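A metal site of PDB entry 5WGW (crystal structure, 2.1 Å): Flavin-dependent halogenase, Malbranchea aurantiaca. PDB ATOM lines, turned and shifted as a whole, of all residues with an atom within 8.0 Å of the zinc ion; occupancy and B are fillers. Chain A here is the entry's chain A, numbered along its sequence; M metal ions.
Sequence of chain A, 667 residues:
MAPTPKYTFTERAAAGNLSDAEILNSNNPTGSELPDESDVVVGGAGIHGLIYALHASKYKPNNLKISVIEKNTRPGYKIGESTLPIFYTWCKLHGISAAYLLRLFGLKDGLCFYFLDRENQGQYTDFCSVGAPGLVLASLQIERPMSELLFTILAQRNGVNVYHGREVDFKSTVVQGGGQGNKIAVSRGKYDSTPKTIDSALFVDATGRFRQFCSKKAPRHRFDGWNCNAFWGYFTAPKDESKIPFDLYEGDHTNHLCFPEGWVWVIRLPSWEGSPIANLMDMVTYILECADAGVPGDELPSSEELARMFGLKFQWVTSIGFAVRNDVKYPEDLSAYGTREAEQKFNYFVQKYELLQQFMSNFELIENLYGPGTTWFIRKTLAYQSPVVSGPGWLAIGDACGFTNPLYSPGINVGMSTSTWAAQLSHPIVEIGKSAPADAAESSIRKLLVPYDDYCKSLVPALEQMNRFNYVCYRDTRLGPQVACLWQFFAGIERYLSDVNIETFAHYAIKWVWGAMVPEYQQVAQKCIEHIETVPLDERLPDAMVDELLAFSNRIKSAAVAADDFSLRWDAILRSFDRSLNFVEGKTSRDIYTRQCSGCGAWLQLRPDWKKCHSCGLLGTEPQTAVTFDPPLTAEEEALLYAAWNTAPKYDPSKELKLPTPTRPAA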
ATOM      1  N   ARG A 268     -23.578  12.521   5.502  1.00  0.00           N
ATOM      2  CA  ARG A 268     -24.147  11.301   4.929  1.00  0.00           C
ATOM      3  C   ARG A 268     -23.092  10.581   4.095  1.00  0.00           C
ATOM      4  O   ARG A 268     -22.497  11.187   3.188  1.00  0.00           O
ATOM      5  CB  ARG A 268     -25.376  11.652   4.084  1.00  0.00           C
ATOM      6  CG  ARG A 268     -26.067  10.451   3.436  1.00  0.00           C
ATOM      7  CD  ARG A 268     -27.092  10.865   2.400  1.00  0.00           C
ATOM      8  NE  ARG A 268     -27.351   9.767   1.475  1.00  0.00           N
ATOM      9  CZ  ARG A 268     -28.398   8.941   1.540  1.00  0.00           C
ATOM     10  NH1 ARG A 268     -29.323   9.114   2.477  1.00  0.00           N
ATOM     11  NH2 ARG A 268     -28.526   7.965   0.663  1.00  0.00           N
ATOM     12  N   SER A 302     -22.641  -0.490  -9.985  1.00  0.00           N
ATOM     13  CA  SER A 302     -23.003   0.375  -8.882  1.00  0.00           C
ATOM     14  C   SER A 302     -22.445  -0.167  -7.569  1.00  0.00           C
ATOM     15  O   SER A 302     -21.997  -1.312  -7.476  1.00  0.00           O
ATOM     16  CB  SER A 302     -24.516   0.545  -8.795  1.00  0.00           C
ATOM     17  OG  SER A 302     -25.127  -0.639  -8.315  1.00  0.00           O
ATOM     18  N   GLU A 304     -23.916  -1.087  -4.785  1.00  0.00           N
ATOM     19  CA  GLU A 304     -24.581  -2.291  -4.317  1.00  0.00           C
ATOM     20  C   GLU A 304     -24.257  -3.490  -5.198  1.00  0.00           C
ATOM     21  O   GLU A 304     -24.169  -4.604  -4.696  1.00  0.00           O
ATOM     22  CB  GLU A 304     -26.094  -2.056  -4.266  1.00  0.00           C
ATOM     23  CG  GLU A 304     -26.503  -0.983  -3.256  1.00  0.00           C
ATOM     24  CD  GLU A 304     -27.985  -0.667  -3.289  1.00  0.00           C
ATOM     25  OE1 GLU A 304     -28.746  -1.417  -3.944  1.00  0.00           O
ATOM     26  OE2 GLU A 304     -28.382   0.346  -2.667  1.00  0.00           O
ATOM     27  N   TRP A 316     -26.046   2.768   4.184  1.00  0.00           N
ATOM     28  CA  TRP A 316     -25.977   4.221   4.290  1.00  0.00           C
ATOM     29  C   TRP A 316     -26.101   4.636   5.750  1.00  0.00           C
ATOM     30  O   TRP A 316     -27.007   4.173   6.452  1.00  0.00           O
ATOM     31  CB  TRP A 316     -27.083   4.888   3.452  1.00  0.00           C
ATOM     32  CG  TRP A 316     -26.734   4.936   1.995  1.00  0.00           C
ATOM     33  CD1 TRP A 316     -27.200   4.116   1.023  1.00  0.00           C
ATOM     34  CD2 TRP A 316     -25.822   5.844   1.372  1.00  0.00           C
ATOM     35  NE1 TRP A 316     -26.635   4.458  -0.194  1.00  0.00           N
ATOM     36  CE2 TRP A 316     -25.789   5.515  -0.003  1.00  0.00           C
ATOM     37  CE3 TRP A 316     -25.033   6.910   1.830  1.00  0.00           C
ATOM     38  CZ2 TRP A 316     -25.006   6.209  -0.919  1.00  0.00           C
ATOM     39  CZ3 TRP A 316     -24.248   7.593   0.924  1.00  0.00           C
ATOM     40  CH2 TRP A 316     -24.237   7.246  -0.437  1.00  0.00           C
ATOM     41  N   ARG A 595     -29.229  15.531  -7.520  1.00  0.00           N
ATOM     42  CA  ARG A 595     -30.575  15.038  -7.294  1.00  0.00           C
ATOM     43  C   ARG A 595     -30.494  13.797  -6.416  1.00  0.00           C
ATOM     44  O   ARG A 595     -29.444  13.148  -6.330  1.00  0.00           O
ATOM     45  CB  ARG A 595     -31.305  14.709  -8.606  1.00  0.00           C
ATOM     46  CG  ARG A 595     -30.796  13.432  -9.265  1.00  0.00           C
ATOM     47  CD  ARG A 595     -31.634  13.054 -10.469  1.00  0.00           C
ATOM     48  NE  ARG A 595     -31.174  11.814 -11.092  1.00  0.00           N
ATOM     49  CZ  ARG A 595     -31.704  10.619 -10.874  1.00  0.00           C
ATOM     50  NH1 ARG A 595     -32.739  10.496 -10.049  1.00  0.00           N
ATOM     51  NH2 ARG A 595     -31.215   9.544 -11.482  1.00  0.00           N
ATOM     52  N   GLN A 596     -31.596  13.469  -5.759  1.00  0.00           N
ATOM     53  CA  GLN A 596     -31.660  12.290  -4.896  1.00  0.00           C
ATOM     54  C   GLN A 596     -32.317  11.149  -5.652  1.00  0.00           C
ATOM     55  O   GLN A 596     -33.406  11.313  -6.218  1.00  0.00           O
ATOM     56  CB  GLN A 596     -32.425  12.597  -3.602  1.00  0.00           C
ATOM     57  CG  GLN A 596     -31.831  11.903  -2.383  1.00  0.00           C
ATOM     58  CD  GLN A 596     -32.664  12.086  -1.127  1.00  0.00           C
ATOM     59  OE1 GLN A 596     -33.606  12.873  -1.091  1.00  0.00           O
ATOM     60  NE2 GLN A 596     -32.313  11.345  -0.078  1.00  0.00           N
ATOM     61  N   CYS A 597     -31.644   9.996  -5.674  1.00  0.00           N
ATOM     62  CA  CYS A 597     -32.196   8.806  -6.300  1.00  0.00           C
ATOM     63  C   CYS A 597     -33.491   8.405  -5.587  1.00  0.00           C
ATOM     64  O   CYS A 597     -33.499   8.230  -4.369  1.00  0.00           O
ATOM     65  CB  CYS A 597     -31.176   7.669  -6.252  1.00  0.00           C
ATOM     66  SG  CYS A 597     -31.754   6.082  -6.935  1.00  0.00           S
ATOM     67  N   SER A 598     -34.574   8.279  -6.349  1.00  0.00           N
ATOM     68  CA  SER A 598     -35.851   7.914  -5.757  1.00  0.00           C
ATOM     69  C   SER A 598     -35.854   6.484  -5.235  1.00  0.00           C
ATOM     70  O   SER A 598     -36.681   6.157  -4.379  1.00  0.00           O
ATOM     71  CB  SER A 598     -36.979   8.109  -6.773  1.00  0.00           C
ATOM     72  OG  SER A 598     -36.714   7.381  -7.964  1.00  0.00           O
ATOM     73  N   GLY A 599     -34.957   5.636  -5.734  1.00  0.00           N
ATOM     74  CA  GLY A 599     -34.923   4.242  -5.345  1.00  0.00           C
ATOM     75  C   GLY A 599     -34.222   3.989  -4.037  1.00  0.00           C
ATOM     76  O   GLY A 599     -34.789   3.367  -3.129  1.00  0.00           O
ATOM     77  N   CYS A 600     -32.980   4.471  -3.906  1.00  0.00           N
ATOM     78  CA  CYS A 600     -32.151   4.162  -2.748  1.00  0.00           C
ATOM     79  C   CYS A 600     -31.862   5.374  -1.862  1.00  0.00           C
ATOM     80  O   CYS A 600     -31.327   5.192  -0.765  1.00  0.00           O
ATOM     81  CB  CYS A 600     -30.825   3.543  -3.192  1.00  0.00           C
ATOM     82  SG  CYS A 600     -29.692   4.719  -3.979  1.00  0.00           S
ATOM     83  N   GLY A 601     -32.192   6.594  -2.309  1.00  0.00           N
ATOM     84  CA  GLY A 601     -31.932   7.787  -1.542  1.00  0.00           C
ATOM     85  C   GLY A 601     -30.555   8.398  -1.721  1.00  0.00           C
ATOM     86  O   GLY A 601     -30.274   9.441  -1.117  1.00  0.00           O
ATOM     87  N   ALA A 602     -29.692   7.794  -2.537  1.00  0.00           N
ATOM     88  CA  ALA A 602     -28.339   8.322  -2.696  1.00  0.00           C
ATOM     89  C   ALA A 602     -28.347   9.585  -3.529  1.00  0.00           C
ATOM     90  O   ALA A 602     -29.112   9.714  -4.494  1.00  0.00           O
ATOM     91  CB  ALA A 602     -27.423   7.280  -3.342  1.00  0.00           C
ATOM     92  N   TRP A 603     -27.480  10.528  -3.173  1.00  0.00           N
ATOM     93  CA  TRP A 603     -27.385  11.780  -3.899  1.00  0.00           C
ATOM     94  C   TRP A 603     -26.448  11.630  -5.094  1.00  0.00           C
ATOM     95  O   TRP A 603     -25.382  11.025  -4.985  1.00  0.00           O
ATOM     96  CB  TRP A 603     -26.915  12.900  -2.972  1.00  0.00           C
ATOM     97  CG  TRP A 603     -28.010  13.347  -2.039  1.00  0.00           C
ATOM     98  CD1 TRP A 603     -28.302  12.839  -0.801  1.00  0.00           C
ATOM     99  CD2 TRP A 603     -28.945  14.398  -2.274  1.00  0.00           C
ATOM    100  NE1 TRP A 603     -29.367  13.515  -0.252  1.00  0.00           N
ATOM    101  CE2 TRP A 603     -29.786  14.478  -1.137  1.00  0.00           C
ATOM    102  CE3 TRP A 603     -29.167  15.280  -3.337  1.00  0.00           C
ATOM    103  CZ2 TRP A 603     -30.824  15.401  -1.035  1.00  0.00           C
ATOM    104  CZ3 TRP A 603     -30.202  16.190  -3.239  1.00  0.00           C
ATOM    105  CH2 TRP A 603     -31.014  16.245  -2.092  1.00  0.00           C
ATOM    106  N   LEU A 604     -26.876  12.170  -6.232  1.00  0.00           N
ATOM    107  CA  LEU A 604     -26.221  11.944  -7.517  1.00  0.00           C
ATOM    108  C   LEU A 604     -25.809  13.270  -8.139  1.00  0.00           C
ATOM    109  O   LEU A 604     -26.450  14.300  -7.920  1.00  0.00           O
ATOM    110  CB  LEU A 604     -27.156  11.192  -8.471  1.00  0.00           C
ATOM    111  CG  LEU A 604     -27.801   9.907  -7.947  1.00  0.00           C
ATOM    112  CD1 LEU A 604     -28.838   9.387  -8.928  1.00  0.00           C
ATOM    113  CD2 LEU A 604     -26.741   8.862  -7.662  1.00  0.00           C
ATOM    114  N   LYS A 612     -27.736   6.408 -14.905  1.00  0.00           N
ATOM    115  CA  LYS A 612     -28.133   5.529 -13.829  1.00  0.00           C
ATOM    116  C   LYS A 612     -27.536   5.977 -12.505  1.00  0.00           C
ATOM    117  O   LYS A 612     -26.485   6.616 -12.458  1.00  0.00           O
ATOM    118  CB  LYS A 612     -27.714   4.078 -14.110  1.00  0.00           C
ATOM    119  CG  LYS A 612     -26.230   3.809 -13.882  1.00  0.00           C
ATOM    120  CD  LYS A 612     -25.904   2.324 -14.018  1.00  0.00           C
ATOM    121  CE  LYS A 612     -24.453   2.045 -13.640  1.00  0.00           C
ATOM    122  NZ  LYS A 612     -24.100   0.610 -13.811  1.00  0.00           N
ATOM    123  N   CYS A 613     -28.238   5.646 -11.422  1.00  0.00           N
ATOM    124  CA  CYS A 613     -27.707   5.869 -10.078  1.00  0.00           C
ATOM    125  C   CYS A 613     -26.415   5.067  -9.891  1.00  0.00           C
ATOM    126  O   CYS A 613     -26.386   3.861 -10.133  1.00  0.00           O
ATOM    127  CB  CYS A 613     -28.751   5.461  -9.036  1.00  0.00           C
ATOM    128  SG  CYS A 613     -28.218   5.514  -7.292  1.00  0.00           S
ATOM    129  N   HIS A 614     -25.351   5.751  -9.486  1.00  0.00           N
ATOM    130  CA  HIS A 614     -24.064   5.086  -9.299  1.00  0.00           C
ATOM    131  C   HIS A 614     -24.040   4.200  -8.064  1.00  0.00           C
ATOM    132  O   HIS A 614     -23.096   3.413  -7.902  1.00  0.00           O
ATOM    133  CB  HIS A 614     -22.934   6.112  -9.215  1.00  0.00           C
ATOM    134  CG  HIS A 614     -22.959   6.950  -7.963  1.00  0.00           C
ATOM    135  ND1 HIS A 614     -23.466   8.228  -7.947  1.00  0.00           N
ATOM    136  CD2 HIS A 614     -22.553   6.682  -6.709  1.00  0.00           C
ATOM    137  CE1 HIS A 614     -23.360   8.720  -6.720  1.00  0.00           C
ATOM    138  NE2 HIS A 614     -22.812   7.798  -5.946  1.00  0.00           N
ATOM    139  N   SER A 615     -25.036   4.301  -7.183  1.00  0.00           N
ATOM    140  CA  SER A 615     -25.050   3.583  -5.930  1.00  0.00           C
ATOM    141  C   SER A 615     -25.924   2.342  -5.949  1.00  0.00           C
ATOM    142  O   SER A 615     -25.536   1.314  -5.378  1.00  0.00           O
ATOM    143  CB  SER A 615     -25.513   4.502  -4.796  1.00  0.00           C
ATOM    144  OG  SER A 615     -25.322   3.896  -3.538  1.00  0.00           O
ATOM    145  N   CYS A 616     -27.084   2.395  -6.592  1.00  0.00           N
ATOM    146  CA  CYS A 616     -27.954   1.230  -6.706  1.00  0.00           C
ATOM    147  C   CYS A 616     -28.207   0.774  -8.133  1.00  0.00           C
ATOM    148  O   CYS A 616     -28.702  -0.341  -8.334  1.00  0.00           O
ATOM    149  CB  CYS A 616     -29.308   1.489  -6.019  1.00  0.00           C
ATOM    150  SG  CYS A 616     -30.526   2.353  -7.024  1.00  0.00           S
ATOM    151  N   GLY A 617     -27.888   1.593  -9.136  1.00  0.00           N
ATOM    152  CA  GLY A 617     -28.023   1.195 -10.518  1.00  0.00           C
ATOM    153  C   GLY A 617     -29.343   1.561 -11.177  1.00  0.00           C
ATOM    154  O   GLY A 617     -29.490   1.343 -12.386  1.00  0.00           O
ATOM    155  N   LEU A 618     -30.295   2.099 -10.428  1.00  0.00           N
ATOM    156  CA  LEU A 618     -31.590   2.467 -10.996  1.00  0.00           C
ATOM    157  C   LEU A 618     -31.431   3.579 -12.026  1.00  0.00           C
ATOM    158  O   LEU A 618     -30.696   4.546 -11.821  1.00  0.00           O
ATOM    159  CB  LEU A 618     -32.551   2.899  -9.891  1.00  0.00           C
ATOM    160  CG  LEU A 618     -33.915   3.468 -10.305  1.00  0.00           C
ATOM    161  CD1 LEU A 618     -34.750   2.430 -11.039  1.00  0.00           C
ATOM    162  CD2 LEU A 618     -34.639   3.999  -9.078  1.00  0.00           C
ATOM    163  N   LEU A 619     -32.146   3.438 -13.140  1.00  0.00           N
ATOM    164  CA  LEU A 619     -32.044   4.379 -14.241  1.00  0.00           C
ATOM    165  C   LEU A 619     -32.898   5.620 -13.983  1.00  0.00           C
ATOM    166  O   LEU A 619     -33.986   5.540 -13.417  1.00  0.00           O
ATOM    167  CB  LEU A 619     -32.485   3.708 -15.546  1.00  0.00           C
ATOM    168  CG  LEU A 619     -32.025   4.328 -16.866  1.00  0.00           C
ATOM    169  CD1 LEU A 619     -30.507   4.305 -16.952  1.00  0.00           C
ATOM    170  CD2 LEU A 619     -32.654   3.583 -18.056  1.00  0.00           C
HETATM  171 ZN    ZN M   1     -30.088   4.580  -6.304  1.00  0.00          ZN
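Four residues have an atom within 4 Å of the zinc ion: Cys 597, Cys 600, Cys 613 and Cys 616.
The nearest printed residue that does not touch the zinc ion is Leu 618 (4.7 Å).
The backbone NH (N) of Cys 613 sits at hydrogen-bond distance from the backbone carbonyl oxygen (O) of Leu 618.
SG of Cys 613 lies close to N of Ser 615 (3.4 Å).
The backbone NH (N) of Gly 599 lies close to the side-chain sulfur (SG) of Cys 597.
The backbone carbonyl oxygen of Ala 602 sits at hydrogen-bond distance from the backbone NH of Cys 597.
SG of Cys 600 sits close to N of Ala 602, 3.4 Å away.
The side-chain sulfur (SG) of Cys 616 lies close to the backbone NH (N) of Leu 618, 3.4 Å away.
SG of Cys 613 binds the zinc ion (2.3 Å).
The zinc ion is bound by the side-chain sulfur (SG) of Cys 597 (2.3 Å).
The zinc ion is bound by SG of Cys 600, at 2.4 Å.
The zinc ion is bound by the side-chain sulfur (SG) of Cys 616, 2.4 Å away.
The zinc ion has four donor atoms within binding distance.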
